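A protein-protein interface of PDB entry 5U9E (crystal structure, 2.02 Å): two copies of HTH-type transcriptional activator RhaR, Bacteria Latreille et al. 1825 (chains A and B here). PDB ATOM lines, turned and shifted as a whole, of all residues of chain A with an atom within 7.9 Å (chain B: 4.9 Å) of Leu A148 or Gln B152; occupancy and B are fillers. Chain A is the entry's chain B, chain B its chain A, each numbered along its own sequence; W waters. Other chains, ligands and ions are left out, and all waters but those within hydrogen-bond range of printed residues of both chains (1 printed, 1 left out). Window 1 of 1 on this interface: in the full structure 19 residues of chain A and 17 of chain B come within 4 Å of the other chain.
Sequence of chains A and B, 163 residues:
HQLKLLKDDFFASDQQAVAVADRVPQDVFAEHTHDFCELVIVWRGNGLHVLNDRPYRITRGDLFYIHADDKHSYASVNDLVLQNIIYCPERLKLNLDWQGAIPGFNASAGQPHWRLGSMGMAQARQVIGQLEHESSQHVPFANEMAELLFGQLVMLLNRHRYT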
ATOM      1  N   VAL A  18      32.826  22.542 -16.419  1.00  0.00           N
ATOM      2  CA  VAL A  18      32.216  23.829 -16.090  1.00  0.00           C
ATOM      3  C   VAL A  18      32.361  24.071 -14.592  1.00  0.00           C
ATOM      4  O   VAL A  18      32.377  23.130 -13.810  1.00  0.00           O
ATOM      5  CB  VAL A  18      30.725  23.888 -16.578  1.00  0.00           C
ATOM      6  CG1 VAL A  18      29.958  22.658 -16.131  1.00  0.00           C
ATOM      7  CG2 VAL A  18      30.011  25.165 -16.125  1.00  0.00           C
ATOM      8  N   LEU A  92      32.959  19.335 -22.589  1.00  0.00           N
ATOM      9  CA  LEU A  92      31.541  19.087 -22.346  1.00  0.00           C
ATOM     10  C   LEU A  92      31.154  17.780 -23.014  1.00  0.00           C
ATOM     11  O   LEU A  92      31.296  17.638 -24.231  1.00  0.00           O
ATOM     12  CB  LEU A  92      30.677  20.244 -22.851  1.00  0.00           C
ATOM     13  CG  LEU A  92      30.839  21.544 -22.072  1.00  0.00           C
ATOM     14  CD1 LEU A  92      30.331  22.749 -22.853  1.00  0.00           C
ATOM     15  CD2 LEU A  92      30.092  21.400 -20.735  1.00  0.00           C
ATOM     16  N   LEU A  94      28.006  16.090 -22.562  1.00  0.00           N
ATOM     17  CA  LEU A  94      26.576  15.929 -22.834  1.00  0.00           C
ATOM     18  C   LEU A  94      26.310  16.302 -24.296  1.00  0.00           C
ATOM     19  O   LEU A  94      26.883  17.274 -24.793  1.00  0.00           O
ATOM     20  CB  LEU A  94      25.775  16.825 -21.881  1.00  0.00           C
ATOM     21  CG  LEU A  94      24.286  16.563 -21.647  1.00  0.00           C
ATOM     22  CD1 LEU A  94      24.071  15.160 -21.045  1.00  0.00           C
ATOM     23  CD2 LEU A  94      23.723  17.653 -20.717  1.00  0.00           C
ATOM     24  N   LEU A  96      24.234  17.887 -25.934  1.00  0.00           N
ATOM     25  CA  LEU A  96      23.444  19.094 -26.153  1.00  0.00           C
ATOM     26  C   LEU A  96      23.992  19.887 -27.331  1.00  0.00           C
ATOM     27  O   LEU A  96      25.169  19.769 -27.682  1.00  0.00           O
ATOM     28  CB  LEU A  96      23.509  19.948 -24.882  1.00  0.00           C
ATOM     29  CG  LEU A  96      22.229  20.516 -24.293  1.00  0.00           C
ATOM     30  CD1 LEU A  96      21.199  19.418 -24.194  1.00  0.00           C
ATOM     31  CD2 LEU A  96      22.523  21.124 -22.936  1.00  0.00           C
ATOM     32  N   TRP A  98      25.323  22.749 -27.770  1.00  0.00           N
ATOM     33  CA  TRP A  98      25.877  23.812 -26.941  1.00  0.00           C
ATOM     34  C   TRP A  98      26.132  25.088 -27.744  1.00  0.00           C
ATOM     35  O   TRP A  98      25.775  26.185 -27.315  1.00  0.00           O
ATOM     36  CB  TRP A  98      27.186  23.357 -26.302  1.00  0.00           C
ATOM     37  CG  TRP A  98      27.071  22.222 -25.311  1.00  0.00           C
ATOM     38  CD1 TRP A  98      27.439  20.911 -25.515  1.00  0.00           C
ATOM     39  CD2 TRP A  98      26.600  22.302 -23.960  1.00  0.00           C
ATOM     40  NE1 TRP A  98      27.214  20.179 -24.372  1.00  0.00           N
ATOM     41  CE2 TRP A  98      26.698  21.006 -23.407  1.00  0.00           C
ATOM     42  CE3 TRP A  98      26.106  23.344 -23.159  1.00  0.00           C
ATOM     43  CZ2 TRP A  98      26.323  20.727 -22.091  1.00  0.00           C
ATOM     44  CZ3 TRP A  98      25.722  23.058 -21.854  1.00  0.00           C
ATOM     45  CH2 TRP A  98      25.834  21.758 -21.334  1.00  0.00           C
ATOM     46  N   VAL A 127      19.746  28.314 -10.466  1.00  0.00           N
ATOM     47  CA  VAL A 127      20.542  27.256 -11.106  1.00  0.00           C
ATOM     48  C   VAL A 127      22.045  27.398 -10.809  1.00  0.00           C
ATOM     49  O   VAL A 127      22.731  26.411 -10.546  1.00  0.00           O
ATOM     50  CB  VAL A 127      20.249  27.203 -12.608  1.00  0.00           C
ATOM     51  CG1 VAL A 127      21.064  26.112 -13.304  1.00  0.00           C
ATOM     52  CG2 VAL A 127      18.768  26.931 -12.806  1.00  0.00           C
ATOM     53  N   GLN A 130      22.788  26.083  -7.452  1.00  0.00           N
ATOM     54  CA  GLN A 130      22.887  24.616  -7.520  1.00  0.00           C
ATOM     55  C   GLN A 130      24.212  24.176  -8.150  1.00  0.00           C
ATOM     56  O   GLN A 130      24.886  23.268  -7.645  1.00  0.00           O
ATOM     57  CB  GLN A 130      21.689  24.014  -8.281  1.00  0.00           C
ATOM     58  CG  GLN A 130      20.314  24.230  -7.591  1.00  0.00           C
ATOM     59  CD  GLN A 130      19.095  23.939  -8.499  1.00  0.00           C
ATOM     60  OE1 GLN A 130      18.220  24.791  -8.671  1.00  0.00           O
ATOM     61  NE2 GLN A 130      19.028  22.729  -9.046  1.00  0.00           N
ATOM     62  N   LEU A 131      24.591  24.830  -9.249  1.00  0.00           N
ATOM     63  CA  LEU A 131      25.815  24.476  -9.967  1.00  0.00           C
ATOM     64  C   LEU A 131      27.042  24.686  -9.078  1.00  0.00           C
ATOM     65  O   LEU A 131      27.984  23.886  -9.105  1.00  0.00           O
ATOM     66  CB  LEU A 131      25.938  25.330 -11.240  1.00  0.00           C
ATOM     67  CG  LEU A 131      27.192  25.242 -12.106  1.00  0.00           C
ATOM     68  CD1 LEU A 131      27.411  23.800 -12.587  1.00  0.00           C
ATOM     69  CD2 LEU A 131      27.067  26.180 -13.320  1.00  0.00           C
ATOM     70  N   GLU A 134      27.737  21.687  -6.984  1.00  0.00           N
ATOM     71  CA  GLU A 134      28.162  20.452  -7.625  1.00  0.00           C
ATOM     72  C   GLU A 134      29.638  20.508  -8.025  1.00  0.00           C
ATOM     73  O   GLU A 134      30.057  19.806  -8.933  1.00  0.00           O
ATOM     74  CB  GLU A 134      27.274  20.106  -8.826  1.00  0.00           C
ATOM     75  CG  GLU A 134      25.821  19.781  -8.447  1.00  0.00           C
ATOM     76  CD  GLU A 134      25.658  18.412  -7.793  1.00  0.00           C
ATOM     77  OE1 GLU A 134      24.533  18.111  -7.336  1.00  0.00           O
ATOM     78  OE2 GLU A 134      26.640  17.621  -7.739  1.00  0.00           O
ATOM     79  N   PHE A 141      28.457  11.437  -9.410  1.00  0.00           N
ATOM     80  CA  PHE A 141      27.727  12.118 -10.474  1.00  0.00           C
ATOM     81  C   PHE A 141      27.790  13.637 -10.436  1.00  0.00           C
ATOM     82  O   PHE A 141      27.015  14.308 -11.128  1.00  0.00           O
ATOM     83  CB  PHE A 141      26.270  11.623 -10.529  1.00  0.00           C
ATOM     84  CG  PHE A 141      26.135  10.133 -10.381  1.00  0.00           C
ATOM     85  CD1 PHE A 141      26.774   9.269 -11.269  1.00  0.00           C
ATOM     86  CD2 PHE A 141      25.375   9.590  -9.350  1.00  0.00           C
ATOM     87  CE1 PHE A 141      26.661   7.894 -11.124  1.00  0.00           C
ATOM     88  CE2 PHE A 141      25.252   8.218  -9.201  1.00  0.00           C
ATOM     89  CZ  PHE A 141      25.892   7.362 -10.075  1.00  0.00           C
ATOM     90  N   ALA A 142      28.704  14.202  -9.652  1.00  0.00           N
ATOM     91  CA  ALA A 142      28.821  15.649  -9.610  1.00  0.00           C
ATOM     92  C   ALA A 142      29.133  16.287 -10.979  1.00  0.00           C
ATOM     93  O   ALA A 142      28.553  17.317 -11.330  1.00  0.00           O
ATOM     94  CB  ALA A 142      29.846  16.083  -8.577  1.00  0.00           C
ATOM     95  N   ASN A 143      30.030  15.672 -11.752  1.00  0.00           N
ATOM     96  CA  ASN A 143      30.394  16.227 -13.053  1.00  0.00           C
ATOM     97  C   ASN A 143      29.221  16.185 -14.016  1.00  0.00           C
ATOM     98  O   ASN A 143      28.963  17.155 -14.721  1.00  0.00           O
ATOM     99  CB  ASN A 143      31.570  15.471 -13.659  1.00  0.00           C
ATOM    100  CG  ASN A 143      32.640  15.163 -12.648  1.00  0.00           C
ATOM    101  OD1 ASN A 143      32.525  14.208 -11.868  1.00  0.00           O
ATOM    102  ND2 ASN A 143      33.692  15.972 -12.642  1.00  0.00           N
ATOM    103  N   GLU A 144      28.524  15.052 -14.043  1.00  0.00           N
ATOM    104  CA  GLU A 144      27.310  14.935 -14.833  1.00  0.00           C
ATOM    105  C   GLU A 144      26.244  15.946 -14.375  1.00  0.00           C
ATOM    106  O   GLU A 144      25.634  16.623 -15.203  1.00  0.00           O
ATOM    107  CB  GLU A 144      26.765  13.501 -14.804  1.00  0.00           C
ATOM    108  CG  GLU A 144      27.695  12.447 -15.446  1.00  0.00           C
ATOM    109  CD  GLU A 144      28.660  11.798 -14.440  1.00  0.00           C
ATOM    110  OE1 GLU A 144      28.975  12.433 -13.409  1.00  0.00           O
ATOM    111  OE2 GLU A 144      29.084  10.647 -14.671  1.00  0.00           O
ATOM    112  N   MET A 145      26.030  16.059 -13.067  1.00  0.00           N
ATOM    113  CA  MET A 145      25.097  17.054 -12.540  1.00  0.00           C
ATOM    114  C   MET A 145      25.513  18.473 -12.970  1.00  0.00           C
ATOM    115  O   MET A 145      24.669  19.283 -13.337  1.00  0.00           O
ATOM    116  CB  MET A 145      25.018  16.990 -11.002  1.00  0.00           C
ATOM    117  CG  MET A 145      24.136  15.885 -10.435  1.00  0.00           C
ATOM    118  SD  MET A 145      22.390  16.051 -10.873  1.00  0.00           S
ATOM    119  CE  MET A 145      22.006  17.651 -10.235  1.00  0.00           C
ATOM    120  N   ALA A 146      26.808  18.778 -12.900  1.00  0.00           N
ATOM    121  CA  ALA A 146      27.284  20.100 -13.315  1.00  0.00           C
ATOM    122  C   ALA A 146      26.919  20.381 -14.775  1.00  0.00           C
ATOM    123  O   ALA A 146      26.435  21.462 -15.086  1.00  0.00           O
ATOM    124  CB  ALA A 146      28.800  20.227 -13.108  1.00  0.00           C
ATOM    125  N   GLU A 147      27.153  19.415 -15.666  1.00  0.00           N
ATOM    126  CA  GLU A 147      26.789  19.599 -17.070  1.00  0.00           C
ATOM    127  C   GLU A 147      25.282  19.751 -17.280  1.00  0.00           C
ATOM    128  O   GLU A 147      24.844  20.563 -18.092  1.00  0.00           O
ATOM    129  CB  GLU A 147      27.305  18.447 -17.950  1.00  0.00           C
ATOM    130  CG  GLU A 147      28.798  18.454 -18.170  1.00  0.00           C
ATOM    131  CD  GLU A 147      29.202  17.822 -19.507  1.00  0.00           C
ATOM    132  OE1 GLU A 147      30.320  17.272 -19.579  1.00  0.00           O
ATOM    133  OE2 GLU A 147      28.410  17.897 -20.475  1.00  0.00           O
ATOM    134  N   LEU A 148      24.491  18.953 -16.560  1.00  0.00           N
ATOM    135  CA  LEU A 148      23.044  19.032 -16.681  1.00  0.00           C
ATOM    136  C   LEU A 148      22.547  20.402 -16.224  1.00  0.00           C
ATOM    137  O   LEU A 148      21.657  21.000 -16.857  1.00  0.00           O
ATOM    138  CB  LEU A 148      22.370  17.910 -15.862  1.00  0.00           C
ATOM    139  CG  LEU A 148      22.605  16.506 -16.428  1.00  0.00           C
ATOM    140  CD1 LEU A 148      22.220  15.426 -15.437  1.00  0.00           C
ATOM    141  CD2 LEU A 148      21.849  16.325 -17.751  1.00  0.00           C
ATOM    142  N   LEU A 149      23.112  20.897 -15.125  1.00  0.00           N
ATOM    143  CA  LEU A 149      22.749  22.220 -14.595  1.00  0.00           C
ATOM    144  C   LEU A 149      23.224  23.352 -15.509  1.00  0.00           C
ATOM    145  O   LEU A 149      22.525  24.349 -15.714  1.00  0.00           O
ATOM    146  CB  LEU A 149      23.319  22.410 -13.184  1.00  0.00           C
ATOM    147  CG  LEU A 149      22.569  21.605 -12.112  1.00  0.00           C
ATOM    148  CD1 LEU A 149      23.436  21.446 -10.875  1.00  0.00           C
ATOM    149  CD2 LEU A 149      21.243  22.302 -11.754  1.00  0.00           C
ATOM    150  N   PHE A 150      24.419  23.202 -16.063  1.00  0.00           N
ATOM    151  CA  PHE A 150      24.929  24.206 -16.994  1.00  0.00           C
ATOM    152  C   PHE A 150      24.055  24.191 -18.248  1.00  0.00           C
ATOM    153  O   PHE A 150      23.731  25.244 -18.819  1.00  0.00           O
ATOM    154  CB  PHE A 150      26.393  23.921 -17.317  1.00  0.00           C
ATOM    155  CG  PHE A 150      27.030  24.927 -18.245  1.00  0.00           C
ATOM    156  CD1 PHE A 150      27.004  26.291 -17.949  1.00  0.00           C
ATOM    157  CD2 PHE A 150      27.702  24.498 -19.384  1.00  0.00           C
ATOM    158  CE1 PHE A 150      27.612  27.221 -18.794  1.00  0.00           C
ATOM    159  CE2 PHE A 150      28.315  25.416 -20.251  1.00  0.00           C
ATOM    160  CZ  PHE A 150      28.283  26.776 -19.952  1.00  0.00           C
ATOM    161  N   GLY A 151      23.647  22.995 -18.665  1.00  0.00           N
ATOM    162  CA  GLY A 151      22.713  22.875 -19.770  1.00  0.00           C
ATOM    163  C   GLY A 151      21.427  23.633 -19.468  1.00  0.00           C
ATOM    164  O   GLY A 151      20.921  24.379 -20.299  1.00  0.00           O
ATOM    165  N   GLN A 152      20.910  23.450 -18.256  1.00  0.00           N
ATOM    166  CA  GLN A 152      19.686  24.123 -17.842  1.00  0.00           C
ATOM    167  C   GLN A 152      19.902  25.645 -17.820  1.00  0.00           C
ATOM    168  O   GLN A 152      19.055  26.410 -18.284  1.00  0.00           O
ATOM    169  CB  GLN A 152      19.251  23.637 -16.441  1.00  0.00           C
ATOM    170  CG  GLN A 152      17.966  24.287 -15.954  1.00  0.00           C
ATOM    171  CD  GLN A 152      17.590  23.913 -14.526  1.00  0.00           C
ATOM    172  OE1 GLN A 152      18.293  23.159 -13.849  1.00  0.00           O
ATOM    173  NE2 GLN A 152      16.471  24.462 -14.056  1.00  0.00           N
ATOM    174  N   LEU A 153      21.036  26.078 -17.273  1.00  0.00           N
ATOM    175  CA  LEU A 153      21.335  27.507 -17.166  1.00  0.00           C
ATOM    176  C   LEU A 153      21.329  28.150 -18.551  1.00  0.00           C
ATOM    177  O   LEU A 153      20.684  29.177 -18.805  1.00  0.00           O
ATOM    178  CB  LEU A 153      22.714  27.715 -16.532  1.00  0.00           C
ATOM    179  CG  LEU A 153      23.203  29.171 -16.512  1.00  0.00           C
ATOM    180  CD1 LEU A 153      22.285  30.027 -15.635  1.00  0.00           C
ATOM    181  CD2 LEU A 153      24.649  29.236 -16.005  1.00  0.00           C
ATOM    182  N   VAL A 154      22.062  27.519 -19.448  1.00  0.00           N
ATOM    183  CA  VAL A 154      22.266  28.045 -20.777  1.00  0.00           C
ATOM    184  C   VAL A 154      20.941  28.158 -21.541  1.00  0.00           C
ATOM    185  O   VAL A 154      20.686  29.153 -22.244  1.00  0.00           O
ATOM    186  CB  VAL A 154      23.296  27.151 -21.458  1.00  0.00           C
ATOM    187  CG1 VAL A 154      23.051  27.040 -22.915  1.00  0.00           C
ATOM    188  CG2 VAL A 154      24.706  27.650 -21.092  1.00  0.00           C
ATOM    189  N   MET A 155      20.080  27.155 -21.373  1.00  0.00           N
ATOM    190  CA  MET A 155      18.756  27.197 -21.981  1.00  0.00           C
ATOM    191  C   MET A 155      17.884  28.285 -21.356  1.00  0.00           C
ATOM    192  O   MET A 155      17.164  28.980 -22.069  1.00  0.00           O
ATOM    193  CB  MET A 155      18.063  25.832 -21.905  1.00  0.00           C
ATOM    194  CG  MET A 155      18.709  24.777 -22.821  1.00  0.00           C
ATOM    195  SD  MET A 155      17.729  23.265 -22.983  1.00  0.00           S
ATOM    196  CE  MET A 155      16.289  23.898 -23.833  1.00  0.00           C
ATOM    197  N   LEU B  94      19.059  12.603 -24.567  1.00  0.00           N
ATOM    198  CA  LEU B  94      20.346  12.911 -23.921  1.00  0.00           C
ATOM    199  C   LEU B  94      21.224  11.666 -23.774  1.00  0.00           C
ATOM    200  O   LEU B  94      20.714  10.577 -23.553  1.00  0.00           O
ATOM    201  CB  LEU B  94      20.116  13.523 -22.534  1.00  0.00           C
ATOM    202  CG  LEU B  94      19.612  14.958 -22.454  1.00  0.00           C
ATOM    203  CD1 LEU B  94      19.368  15.330 -20.989  1.00  0.00           C
ATOM    204  CD2 LEU B  94      20.601  15.932 -23.121  1.00  0.00           C
ATOM    205  N   LEU B  96      22.894  10.368 -21.400  1.00  0.00           N
ATOM    206  CA  LEU B  96      23.155   9.826 -20.063  1.00  0.00           C
ATOM    207  C   LEU B  96      22.979   8.335 -20.155  1.00  0.00           C
ATOM    208  O   LEU B  96      22.269   7.843 -21.053  1.00  0.00           O
ATOM    209  CB  LEU B  96      22.168  10.369 -19.028  1.00  0.00           C
ATOM    210  CG  LEU B  96      22.256  11.868 -18.778  1.00  0.00           C
ATOM    211  CD1 LEU B  96      21.168  12.292 -17.783  1.00  0.00           C
ATOM    212  CD2 LEU B  96      23.641  12.222 -18.259  1.00  0.00           C
ATOM    213  N   VAL B 127      13.909  19.604  -8.044  1.00  0.00           N
ATOM    214  CA  VAL B 127      13.924  19.273  -9.466  1.00  0.00           C
ATOM    215  C   VAL B 127      12.531  18.985 -10.017  1.00  0.00           C
ATOM    216  O   VAL B 127      12.156  19.493 -11.074  1.00  0.00           O
ATOM    217  CB  VAL B 127      14.857  18.084  -9.748  1.00  0.00           C
ATOM    218  CG1 VAL B 127      14.628  17.576 -11.142  1.00  0.00           C
ATOM    219  CG2 VAL B 127      16.294  18.536  -9.596  1.00  0.00           C
ATOM    220  N   LEU B 148      16.551  17.632 -19.457  1.00  0.00           N
ATOM    221  CA  LEU B 148      17.702  17.969 -18.615  1.00  0.00           C
ATOM    222  C   LEU B 148      17.335  17.833 -17.132  1.00  0.00           C
ATOM    223  O   LEU B 148      18.122  17.328 -16.334  1.00  0.00           O
ATOM    224  CB  LEU B 148      18.175  19.398 -18.889  1.00  0.00           C
ATOM    225  CG  LEU B 148      18.863  19.679 -20.224  1.00  0.00           C
ATOM    226  CD1 LEU B 148      18.948  21.178 -20.466  1.00  0.00           C
ATOM    227  CD2 LEU B 148      20.253  19.061 -20.198  1.00  0.00           C
ATOM    228  N   LEU B 149      16.139  18.300 -16.773  1.00  0.00           N
ATOM    229  CA  LEU B 149      15.654  18.181 -15.403  1.00  0.00           C
ATOM    230  C   LEU B 149      15.427  16.713 -15.029  1.00  0.00           C
ATOM    231  O   LEU B 149      15.732  16.290 -13.910  1.00  0.00           O
ATOM    232  CB  LEU B 149      14.350  18.995 -15.220  1.00  0.00           C
ATOM    233  CG  LEU B 149      14.616  20.515 -15.191  1.00  0.00           C
ATOM    234  CD1 LEU B 149      13.316  21.326 -15.384  1.00  0.00           C
ATOM    235  CD2 LEU B 149      15.367  20.963 -13.909  1.00  0.00           C
ATOM    236  N   PHE B 150      14.875  15.946 -15.963  1.00  0.00           N
ATOM    237  CA  PHE B 150      14.694  14.521 -15.744  1.00  0.00           C
ATOM    238  C   PHE B 150      16.064  13.855 -15.552  1.00  0.00           C
ATOM    239  O   PHE B 150      16.235  13.004 -14.669  1.00  0.00           O
ATOM    240  CB  PHE B 150      13.943  13.877 -16.920  1.00  0.00           C
ATOM    241  CG  PHE B 150      13.679  12.401 -16.724  1.00  0.00           C
ATOM    242  CD1 PHE B 150      12.815  11.970 -15.727  1.00  0.00           C
ATOM    243  CD2 PHE B 150      14.301  11.454 -17.514  1.00  0.00           C
ATOM    244  CE1 PHE B 150      12.564  10.612 -15.522  1.00  0.00           C
ATOM    245  CE2 PHE B 150      14.038  10.077 -17.323  1.00  0.00           C
ATOM    246  CZ  PHE B 150      13.184   9.666 -16.320  1.00  0.00           C
ATOM    247  N   GLY B 151      17.052  14.260 -16.352  1.00  0.00           N
ATOM    248  CA  GLY B 151      18.405  13.770 -16.134  1.00  0.00           C
ATOM    249  C   GLY B 151      18.932  14.079 -14.726  1.00  0.00           C
ATOM    250  O   GLY B 151      19.535  13.235 -14.075  1.00  0.00           O
ATOM    251  N   GLN B 152      18.717  15.302 -14.261  1.00  0.00           N
ATOM    252  CA  GLN B 152      19.147  15.670 -12.908  1.00  0.00           C
ATOM    253  C   GLN B 152      18.469  14.792 -11.849  1.00  0.00           C
ATOM    254  O   GLN B 152      19.108  14.354 -10.913  1.00  0.00           O
ATOM    255  CB  GLN B 152      18.819  17.136 -12.632  1.00  0.00           C
ATOM    256  CG  GLN B 152      19.660  18.150 -13.426  1.00  0.00           C
ATOM    257  CD  GLN B 152      19.180  19.566 -13.201  1.00  0.00           C
ATOM    258  OE1 GLN B 152      18.775  19.917 -12.082  1.00  0.00           O
ATOM    259  NE2 GLN B 152      19.174  20.383 -14.270  1.00  0.00           N
ATOM    260  N   LEU B 153      17.167  14.561 -11.999  1.00  0.00           N
ATOM    261  CA  LEU B 153      16.408  13.747 -11.052  1.00  0.00           C
ATOM    262  C   LEU B 153      16.974  12.327 -11.013  1.00  0.00           C
ATOM    263  O   LEU B 153      17.232  11.758  -9.960  1.00  0.00           O
ATOM    264  CB  LEU B 153      14.935  13.687 -11.484  1.00  0.00           C
ATOM    265  CG  LEU B 153      14.033  12.779 -10.632  1.00  0.00           C
ATOM    266  CD1 LEU B 153      14.059  13.266  -9.189  1.00  0.00           C
ATOM    267  CD2 LEU B 153      12.568  12.743 -11.185  1.00  0.00           C
ATOM    268  N   VAL B 154      17.169  11.756 -12.186  1.00  0.00           N
ATOM    269  CA  VAL B 154      17.674  10.387 -12.289  1.00  0.00           C
ATOM    270  C   VAL B 154      19.051  10.245 -11.617  1.00  0.00           C
ATOM    271  O   VAL B 154      19.273   9.290 -10.879  1.00  0.00           O
ATOM    272  CB  VAL B 154      17.700   9.956 -13.783  1.00  0.00           C
ATOM    273  CG1 VAL B 154      18.574   8.735 -14.000  1.00  0.00           C
ATOM    274  CG2 VAL B 154      16.261   9.713 -14.271  1.00  0.00           C
ATOM    275  N   MET B 155      19.955  11.201 -11.851  1.00  0.00           N
ATOM    276  CA  MET B 155      21.277  11.184 -11.220  1.00  0.00           C
ATOM    277  C   MET B 155      21.152  11.368  -9.706  1.00  0.00           C
ATOM    278  O   MET B 155      21.819  10.693  -8.939  1.00  0.00           O
ATOM    279  CB  MET B 155      22.179  12.308 -11.768  1.00  0.00           C
ATOM    280  CG  MET B 155      22.480  12.253 -13.277  1.00  0.00           C
ATOM    281  SD  MET B 155      23.526  10.865 -13.750  1.00  0.00           S
ATOM    282  CE  MET B 155      22.285   9.764 -14.230  1.00  0.00           C
ATOM    283  N   LEU B 156      20.320  12.306  -9.291  1.00  0.00           N
ATOM    284  CA  LEU B 156      20.088  12.542  -7.859  1.00  0.00           C
ATOM    285  C   LEU B 156      19.503  11.305  -7.173  1.00  0.00           C
ATOM    286  O   LEU B 156      19.927  10.933  -6.077  1.00  0.00           O
ATOM    287  CB  LEU B 156      19.154  13.728  -7.664  1.00  0.00           C
ATOM    288  CG  LEU B 156      19.768  15.105  -7.856  1.00  0.00           C
ATOM    289  CD1 LEU B 156      18.634  16.146  -7.914  1.00  0.00           C
ATOM    290  CD2 LEU B 156      20.756  15.418  -6.716  1.00  0.00           C
ATOM    291  N   LEU B 157      18.544  10.655  -7.823  1.00  0.00           N
ATOM    292  CA  LEU B 157      18.007   9.403  -7.279  1.00  0.00           C
ATOM    293  C   LEU B 157      19.095   8.349  -7.156  1.00  0.00           C
ATOM    294  O   LEU B 157      19.181   7.666  -6.142  1.00  0.00           O
ATOM    295  CB  LEU B 157      16.838   8.885  -8.124  1.00  0.00           C
ATOM    296  CG  LEU B 157      15.603   9.803  -8.092  1.00  0.00           C
ATOM    297  CD1 LEU B 157      14.477   9.229  -8.931  1.00  0.00           C
ATOM    298  CD2 LEU B 157      15.102  10.024  -6.669  1.00  0.00           C
HETATM  299  O   HOH W   1      17.183  21.953 -11.037  1.00  0.00           O
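Of the printed residues of chain B, Leu A148 touches Gly B151 (3.6 Å), Gln B152 (3.6 Å) and Met B155 (3.8 Å). Of the printed residues of chain B, Gly A151 touches Leu B148. Printed residues of chain B within 4 Å of Met A155: Leu B148. Of the printed residues of chain A, Leu B149 touches Gln A152. Of chain A, only Leu A148 (3.6 Å) comes within 4 Å of Gly B151. Of the printed residues of chain A, Gln B152 touches Met A145, Leu A148, Leu A149 and Gln A152. The nearest printed residue of chain B that does not touch Leu A148 is Leu B148 (4.003 Å).
Of the 24 printed residues of chain A, 9 touch a printed residue of chain B. Hydrophobic or aromatic side chains of chain A that line the printed part of chain B: Leu A94, Leu A96, Phe A141, Met A145, Leu A148, Leu A149 and Met A155. Hydrophobic or aromatic side chains of chain B within 4 Å of the printed part of chain A: Leu B94, Leu B148, Leu B149 and Met B155. Among the printed residues, no Asp or Glu carboxylate lies within 4 Å of a Lys or Arg side-chain nitrogen of the other chain.
OE2 of Glu A147 lies within hydrogen-bond range of N of Leu A94 (2.8 Å). O of Leu A94 lies within hydrogen-bond range of NE1 of Trp A98.
NE2 of Gln B152 lies within hydrogen-bond range of OE1 of Gln A152 (2.9 Å). O of Gln B152 sits close to SD of Met A145, at 3.7 Å.
Among the printed residues, merely in contact across the chains: Leu A149 with Gln B152 (3.4 Å), Met A155 with Leu B148 (3.5 Å), Leu A148 with Gly B151 (3.6 Å), Gly A151 with Leu B148 (3.6 Å), Leu A148 with Gln B152 (3.6 Å), Gln A152 with Leu B149 (3.7 Å), Leu A96 with Leu B94 (3.7 Å), Gln A152 with Leu B148 (3.7 Å), Phe A141 with Met B155 (3.7 Å), Leu A94 with Leu B148 (3.8 Å), Leu A148 with Met B155 (3.8 Å) and Met A145 with Met B155 (3.9 Å).
Leu A148 touches Gly B151, and with the chains exchanged Gly A151 touches Leu B148. Leu A148 touches Gln B152, and with the chains exchanged Gln A152 touches Leu B148. Leu A149 touches Gln B152, and with the chains exchanged Gln A152 touches Leu B149. Gln B152 touches its own counterpart, Gln A152. Of the 14 pairs that touch across the chains among the printed residues, 9 have their exchanged pair printed and touching as well.
Water W1 lies within hydrogen-bond range of OE1 of Gln B152 (2.8 Å), NE2 of Gln A130 (2.8 Å) and OE1 of Gln A152 (3.3 Å).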
